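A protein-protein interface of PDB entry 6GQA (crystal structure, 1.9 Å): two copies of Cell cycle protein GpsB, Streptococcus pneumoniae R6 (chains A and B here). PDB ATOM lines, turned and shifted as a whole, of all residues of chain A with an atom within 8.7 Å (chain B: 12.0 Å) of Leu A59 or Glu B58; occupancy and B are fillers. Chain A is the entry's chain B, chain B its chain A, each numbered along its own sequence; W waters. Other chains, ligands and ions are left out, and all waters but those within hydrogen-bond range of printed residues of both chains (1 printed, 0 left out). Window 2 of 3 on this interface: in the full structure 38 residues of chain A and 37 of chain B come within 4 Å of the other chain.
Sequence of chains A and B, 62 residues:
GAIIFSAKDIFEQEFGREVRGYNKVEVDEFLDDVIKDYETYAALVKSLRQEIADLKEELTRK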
ATOM      1  N   ILE A  52     -15.020 -16.843  -0.046  1.00  0.00           N
ATOM      2  CA  ILE A  52     -16.117 -17.280   0.832  1.00  0.00           C
ATOM      3  C   ILE A  52     -15.632 -17.410   2.272  1.00  0.00           C
ATOM      4  O   ILE A  52     -16.284 -16.963   3.222  1.00  0.00           O
ATOM      5  CB  ILE A  52     -16.673 -18.614   0.302  1.00  0.00           C
ATOM      6  CG1 ILE A  52     -17.339 -18.377  -1.071  1.00  0.00           C
ATOM      7  CG2 ILE A  52     -17.431 -19.414   1.412  1.00  0.00           C
ATOM      8  CD1 ILE A  52     -17.486 -19.618  -1.967  1.00  0.00           C
ATOM      9  N   ALA A  53     -14.495 -18.079   2.459  1.00  0.00           N
ATOM     10  CA  ALA A  53     -13.971 -18.275   3.806  1.00  0.00           C
ATOM     11  C   ALA A  53     -13.673 -16.937   4.472  1.00  0.00           C
ATOM     12  O   ALA A  53     -13.947 -16.751   5.670  1.00  0.00           O
ATOM     13  CB  ALA A  53     -12.730 -19.163   3.739  1.00  0.00           C
ATOM     14  N   ASP A  54     -13.136 -15.972   3.717  1.00  0.00           N
ATOM     15  CA  ASP A  54     -12.878 -14.654   4.314  1.00  0.00           C
ATOM     16  C   ASP A  54     -14.182 -13.938   4.658  1.00  0.00           C
ATOM     17  O   ASP A  54     -14.287 -13.274   5.695  1.00  0.00           O
ATOM     18  CB  ASP A  54     -12.055 -13.775   3.366  1.00  0.00           C
ATOM     19  CG  ASP A  54     -10.643 -14.295   3.133  1.00  0.00           C
ATOM     20  OD1 ASP A  54     -10.194 -15.213   3.865  1.00  0.00           O
ATOM     21  OD2 ASP A  54      -9.988 -13.759   2.211  1.00  0.00           O
ATOM     22  N   LEU A  55     -15.185 -14.056   3.791  1.00  0.00           N
ATOM     23  CA  LEU A  55     -16.448 -13.364   4.018  1.00  0.00           C
ATOM     24  C   LEU A  55     -17.219 -13.961   5.187  1.00  0.00           C
ATOM     25  O   LEU A  55     -17.828 -13.221   5.973  1.00  0.00           O
ATOM     26  CB  LEU A  55     -17.282 -13.410   2.746  1.00  0.00           C
ATOM     27  CG  LEU A  55     -16.848 -12.571   1.513  1.00  0.00           C
ATOM     28  CD1 LEU A  55     -17.612 -13.098   0.327  1.00  0.00           C
ATOM     29  CD2 LEU A  55     -17.132 -11.049   1.813  1.00  0.00           C
ATOM     30  N   LYS A  56     -17.233 -15.290   5.298  1.00  0.00           N
ATOM     31  CA  LYS A  56     -17.823 -15.950   6.465  1.00  0.00           C
ATOM     32  C   LYS A  56     -17.137 -15.528   7.752  1.00  0.00           C
ATOM     33  O   LYS A  56     -17.792 -15.277   8.775  1.00  0.00           O
ATOM     34  CB  LYS A  56     -17.723 -17.450   6.301  1.00  0.00           C
ATOM     35  CG  LYS A  56     -18.817 -18.069   5.460  1.00  0.00           C
ATOM     36  CD  LYS A  56     -18.667 -19.568   5.471  1.00  0.00           C
ATOM     37  CE  LYS A  56     -19.825 -20.264   4.788  1.00  0.00           C
ATOM     38  NZ  LYS A  56     -19.909 -19.913   3.346  1.00  0.00           N
ATOM     39  N   GLU A  57     -15.809 -15.482   7.738  1.00  0.00           N
ATOM     40  CA  GLU A  57     -15.078 -15.014   8.913  1.00  0.00           C
ATOM     41  C   GLU A  57     -15.370 -13.539   9.205  1.00  0.00           C
ATOM     42  O   GLU A  57     -15.459 -13.143  10.370  1.00  0.00           O
ATOM     43  CB  GLU A  57     -13.592 -15.275   8.701  1.00  0.00           C
ATOM     44  CG  GLU A  57     -12.631 -14.747   9.746  1.00  0.00           C
ATOM     45  CD  GLU A  57     -11.204 -15.024   9.301  1.00  0.00           C
ATOM     46  OE1 GLU A  57     -10.669 -14.245   8.463  1.00  0.00           O
ATOM     47  OE2 GLU A  57     -10.648 -16.064   9.722  1.00  0.00           O
ATOM     48  N   GLU A  58     -15.546 -12.713   8.164  1.00  0.00           N
ATOM     49  CA  GLU A  58     -15.967 -11.327   8.365  1.00  0.00           C
ATOM     50  C   GLU A  58     -17.321 -11.260   9.061  1.00  0.00           C
ATOM     51  O   GLU A  58     -17.439 -10.713  10.162  1.00  0.00           O
ATOM     52  CB  GLU A  58     -16.019 -10.585   7.029  1.00  0.00           C
ATOM     53  CG  GLU A  58     -14.875  -9.592   6.821  1.00  0.00           C
ATOM     54  CD  GLU A  58     -14.431  -9.502   5.364  1.00  0.00           C
ATOM     55  OE1 GLU A  58     -15.200  -8.956   4.535  1.00  0.00           O
ATOM     56  OE2 GLU A  58     -13.315  -9.999   5.051  1.00  0.00           O
ATOM     57  N   LEU A  59     -18.349 -11.851   8.440  1.00  0.00           N
ATOM     58  CA  LEU A  59     -19.676 -12.090   9.032  1.00  0.00           C
ATOM     59  C   LEU A  59     -19.606 -12.510  10.511  1.00  0.00           C
ATOM     60  O   LEU A  59     -20.441 -12.117  11.339  1.00  0.00           O
ATOM     61  CB  LEU A  59     -20.382 -13.157   8.185  1.00  0.00           C
ATOM     62  CG  LEU A  59     -21.871 -13.207   7.820  1.00  0.00           C
ATOM     63  CD1 LEU A  59     -22.581 -11.868   7.619  1.00  0.00           C
ATOM     64  CD2 LEU A  59     -22.005 -13.999   6.560  1.00  0.00           C
ATOM     65  N   THR A  60     -18.610 -13.319  10.858  1.00  0.00           N
ATOM     66  CA  THR A  60     -18.248 -13.504  12.268  1.00  0.00           C
ATOM     67  C   THR A  60     -17.351 -12.354  12.748  1.00  0.00           C
ATOM     68  O   THR A  60     -17.432 -11.915  13.890  1.00  0.00           O
ATOM     69  CB  THR A  60     -17.535 -14.833  12.469  1.00  0.00           C
ATOM     70  OG1 THR A  60     -18.424 -15.880  12.093  1.00  0.00           O
ATOM     71  CG2 THR A  60     -17.152 -15.041  13.918  1.00  0.00           C
ATOM     72  N   ARG B  49     -19.866 -18.345  -7.045  1.00  0.00           N
ATOM     73  CA  ARG B  49     -20.184 -16.931  -7.236  1.00  0.00           C
ATOM     74  C   ARG B  49     -21.539 -16.608  -6.632  1.00  0.00           C
ATOM     75  O   ARG B  49     -21.736 -15.511  -6.090  1.00  0.00           O
ATOM     76  CB  ARG B  49     -20.126 -16.551  -8.731  1.00  0.00           C
ATOM     77  CG  ARG B  49     -18.695 -16.670  -9.341  1.00  0.00           C
ATOM     78  CD  ARG B  49     -18.626 -15.903 -10.697  1.00  0.00           C
ATOM     79  NE  ARG B  49     -17.276 -15.935 -11.306  1.00  0.00           N
ATOM     80  CZ  ARG B  49     -16.210 -15.295 -10.834  1.00  0.00           C
ATOM     81  NH1 ARG B  49     -16.278 -14.566  -9.736  1.00  0.00           N
ATOM     82  NH2 ARG B  49     -15.062 -15.402 -11.467  1.00  0.00           N
ATOM     83  N   GLN B  50     -22.467 -17.569  -6.629  1.00  0.00           N
ATOM     84  CA  GLN B  50     -23.720 -17.320  -5.928  1.00  0.00           C
ATOM     85  C   GLN B  50     -23.525 -17.269  -4.416  1.00  0.00           C
ATOM     86  O   GLN B  50     -24.089 -16.384  -3.747  1.00  0.00           O
ATOM     87  CB  GLN B  50     -24.748 -18.376  -6.302  1.00  0.00           C
ATOM     88  CG  GLN B  50     -26.197 -17.991  -5.859  1.00  0.00           C
ATOM     89  CD  GLN B  50     -26.711 -16.633  -6.415  1.00  0.00           C
ATOM     90  OE1 GLN B  50     -26.764 -16.411  -7.641  1.00  0.00           O
ATOM     91  NE2 GLN B  50     -27.121 -15.735  -5.502  1.00  0.00           N
ATOM     92  N   GLU B  51     -22.756 -18.207  -3.834  1.00  0.00           N
ATOM     93  CA  GLU B  51     -22.550 -18.138  -2.386  1.00  0.00           C
ATOM     94  C   GLU B  51     -21.922 -16.804  -2.009  1.00  0.00           C
ATOM     95  O   GLU B  51     -22.324 -16.169  -1.037  1.00  0.00           O
ATOM     96  CB  GLU B  51     -21.668 -19.282  -1.865  1.00  0.00           C
ATOM     97  CG  GLU B  51     -22.231 -20.696  -1.910  1.00  0.00           C
ATOM     98  CD  GLU B  51     -21.251 -21.691  -1.360  1.00  0.00           C
ATOM     99  OE1 GLU B  51     -21.006 -22.708  -2.041  1.00  0.00           O
ATOM    100  OE2 GLU B  51     -20.720 -21.464  -0.246  1.00  0.00           O
ATOM    101  N   ILE B  52     -20.931 -16.364  -2.785  1.00  0.00           N
ATOM    102  CA  ILE B  52     -20.331 -15.053  -2.571  1.00  0.00           C
ATOM    103  C   ILE B  52     -21.369 -13.917  -2.673  1.00  0.00           C
ATOM    104  O   ILE B  52     -21.397 -13.018  -1.826  1.00  0.00           O
ATOM    105  CB  ILE B  52     -19.182 -14.856  -3.575  1.00  0.00           C
ATOM    106  CG1 ILE B  52     -18.009 -15.765  -3.209  1.00  0.00           C
ATOM    107  CG2 ILE B  52     -18.869 -13.376  -3.663  1.00  0.00           C
ATOM    108  CD1 ILE B  52     -16.944 -15.953  -4.371  1.00  0.00           C
ATOM    109  N   ALA B  53     -22.237 -13.925  -3.692  1.00  0.00           N
ATOM    110  CA  ALA B  53     -23.210 -12.829  -3.780  1.00  0.00           C
ATOM    111  C   ALA B  53     -24.125 -12.816  -2.551  1.00  0.00           C
ATOM    112  O   ALA B  53     -24.419 -11.747  -1.977  1.00  0.00           O
ATOM    113  CB  ALA B  53     -24.039 -12.933  -5.067  1.00  0.00           C
ATOM    114  N   ASP B  54     -24.564 -14.001  -2.120  1.00  0.00           N
ATOM    115  CA  ASP B  54     -25.448 -14.093  -0.957  1.00  0.00           C
ATOM    116  C   ASP B  54     -24.747 -13.628   0.309  1.00  0.00           C
ATOM    117  O   ASP B  54     -25.369 -12.962   1.142  1.00  0.00           O
ATOM    118  CB  ASP B  54     -25.962 -15.528  -0.773  1.00  0.00           C
ATOM    119  CG  ASP B  54     -26.884 -15.991  -1.916  1.00  0.00           C
ATOM    120  OD1 ASP B  54     -27.358 -15.144  -2.718  1.00  0.00           O
ATOM    121  OD2 ASP B  54     -27.140 -17.214  -1.999  1.00  0.00           O
ATOM    122  N   LEU B  55     -23.476 -14.027   0.520  1.00  0.00           N
ATOM    123  CA  LEU B  55     -22.759 -13.549   1.712  1.00  0.00           C
ATOM    124  C   LEU B  55     -22.632 -12.020   1.706  1.00  0.00           C
ATOM    125  O   LEU B  55     -22.847 -11.364   2.744  1.00  0.00           O
ATOM    126  CB  LEU B  55     -21.383 -14.180   1.823  1.00  0.00           C
ATOM    127  CG  LEU B  55     -21.409 -15.628   2.299  1.00  0.00           C
ATOM    128  CD1 LEU B  55     -20.353 -16.468   1.699  1.00  0.00           C
ATOM    129  CD2 LEU B  55     -21.282 -15.655   3.792  1.00  0.00           C
ATOM    130  N   LYS B  56     -22.276 -11.440   0.540  1.00  0.00           N
ATOM    131  CA  LYS B  56     -22.235  -9.977   0.405  1.00  0.00           C
ATOM    132  C   LYS B  56     -23.581  -9.328   0.714  1.00  0.00           C
ATOM    133  O   LYS B  56     -23.627  -8.280   1.367  1.00  0.00           O
ATOM    134  CB  LYS B  56     -21.780  -9.559  -0.996  1.00  0.00           C
ATOM    135  CG  LYS B  56     -20.319  -9.878  -1.297  1.00  0.00           C
ATOM    136  CD  LYS B  56     -19.886  -9.415  -2.690  1.00  0.00           C
ATOM    137  CE  LYS B  56     -18.351  -9.570  -2.837  1.00  0.00           C
ATOM    138  NZ  LYS B  56     -17.807  -9.139  -4.187  1.00  0.00           N
ATOM    139  N   GLU B  57     -24.690  -9.908   0.250  1.00  0.00           N
ATOM    140  CA  GLU B  57     -25.981  -9.362   0.677  1.00  0.00           C
ATOM    141  C   GLU B  57     -26.097  -9.387   2.205  1.00  0.00           C
ATOM    142  O   GLU B  57     -26.446  -8.381   2.841  1.00  0.00           O
ATOM    143  CB  GLU B  57     -27.135 -10.141   0.032  1.00  0.00           C
ATOM    144  CG  GLU B  57     -27.734  -9.562  -1.252  1.00  0.00           C
ATOM    145  CD  GLU B  57     -28.641 -10.572  -1.964  1.00  0.00           C
ATOM    146  OE1 GLU B  57     -28.879 -11.664  -1.388  1.00  0.00           O
ATOM    147  OE2 GLU B  57     -29.109 -10.296  -3.095  1.00  0.00           O
ATOM    148  N   GLU B  58     -25.731 -10.515   2.816  1.00  0.00           N
ATOM    149  CA  GLU B  58     -25.850 -10.681   4.260  1.00  0.00           C
ATOM    150  C   GLU B  58     -24.899  -9.769   5.034  1.00  0.00           C
ATOM    151  O   GLU B  58     -25.230  -9.329   6.147  1.00  0.00           O
ATOM    152  CB  GLU B  58     -25.607 -12.147   4.605  1.00  0.00           C
ATOM    153  CG  GLU B  58     -25.836 -12.490   6.036  1.00  0.00           C
ATOM    154  CD  GLU B  58     -25.908 -13.975   6.217  1.00  0.00           C
ATOM    155  OE1 GLU B  58     -25.439 -14.699   5.295  1.00  0.00           O
ATOM    156  OE2 GLU B  58     -26.434 -14.419   7.268  1.00  0.00           O
ATOM    157  N   LEU B  59     -23.730  -9.453   4.483  1.00  0.00           N
ATOM    158  CA  LEU B  59     -22.863  -8.517   5.189  1.00  0.00           C
ATOM    159  C   LEU B  59     -23.450  -7.096   5.213  1.00  0.00           C
ATOM    160  O   LEU B  59     -23.101  -6.303   6.099  1.00  0.00           O
ATOM    161  CB  LEU B  59     -21.460  -8.575   4.574  1.00  0.00           C
ATOM    162  CG  LEU B  59     -20.541  -9.730   5.029  1.00  0.00           C
ATOM    163  CD1 LEU B  59     -19.479 -10.071   4.005  1.00  0.00           C
ATOM    164  CD2 LEU B  59     -19.853  -9.395   6.350  1.00  0.00           C
ATOM    165  N   THR B  60     -24.362  -6.770   4.292  1.00  0.00           N
ATOM    166  CA  THR B  60     -25.243  -5.591   4.449  1.00  0.00           C
ATOM    167  C   THR B  60     -26.588  -5.946   5.135  1.00  0.00           C
ATOM    168  O   THR B  60     -26.729  -5.984   6.360  1.00  0.00           O
ATOM    169  CB  THR B  60     -25.566  -4.929   3.068  1.00  0.00           C
ATOM    170  OG1 THR B  60     -26.768  -5.499   2.534  1.00  0.00           O
ATOM    171  CG2 THR B  60     -24.453  -5.165   2.082  1.00  0.00           C
HETATM  172  O   HOH W   1     -21.349 -22.984   2.541  1.00  0.00           O
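The side-chain carboxylate (OE2) of Glu B51 is in salt-bridge range of the side-chain amino group (NZ) of Lys A56 (3.996 Å).
The side-chain hydroxyl of Thr A60 is in hydrogen-bond range of the backbone carbonyl oxygen of Lys A56 (3.4 Å).
CG1 of Ile A52 touches CG1 of Ile B52 (3.4 Å).
Leu A55 touches Leu B59 (CD2 to CD1, 3.4 Å).
CG of Lys A56 touches CD2 of Leu B55, 3.8 Å away.
CD2 of Leu A59 touches CD2 of Leu B55 (3.3 Å).
Glu B58 touches Leu A59.
Leu A59 touches Leu B59 (N to CD2, 3.6 Å).
Leu A55 touches just one residue of chain B: Leu B59.
Of the printed residues of chain B, Lys A56 touches Glu B51 and Leu B55.
No residue of chain B comes within 4 Å of Glu A58.
Of chain B, only Leu B55 (3.3 Å), Glu B58 (3.7 Å) and Leu B59 (3.6 Å) come within 4 Å of Leu A59.
No residue of chain B comes within 4 Å of Thr A60.
Printed residues of chain A within 4 Å of Glu B51: Lys A56.
Asp B54 touches none of the printed residues of chain A.
Glu B58 touches one residue of chain A.
Of the printed residues of chain A, Leu B59 touches Leu A55 (3.4 Å) and Leu A59 (3.6 Å).
Thr B60 touches none of the printed residues of chain A.
The nearest printed residue of chain B that does not touch Lys A56 is Leu B59 (5.8 Å).
Of the 12 printed residues of chain B, 5 touch a printed residue of chain A.
Among the printed residues, 7 pairs touch across the chains.
Leu A55 touches Leu B59, and with the chains exchanged Leu A59 touches Leu B55.
Lys A56 touches Leu B55, but with the chains exchanged Leu A55 does not touch Lys B56 (4.5 Å).
Leu A59 touches Glu B58, but with the chains exchanged Glu A58 does not touch Leu B59 (4.1 Å).
Leu A59 touches its own counterpart, Leu B59.
9 positions are printed for both chains.
Water W1 lies within hydrogen-bond range of OE2 of Glu B51 and NZ of Lys A56.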
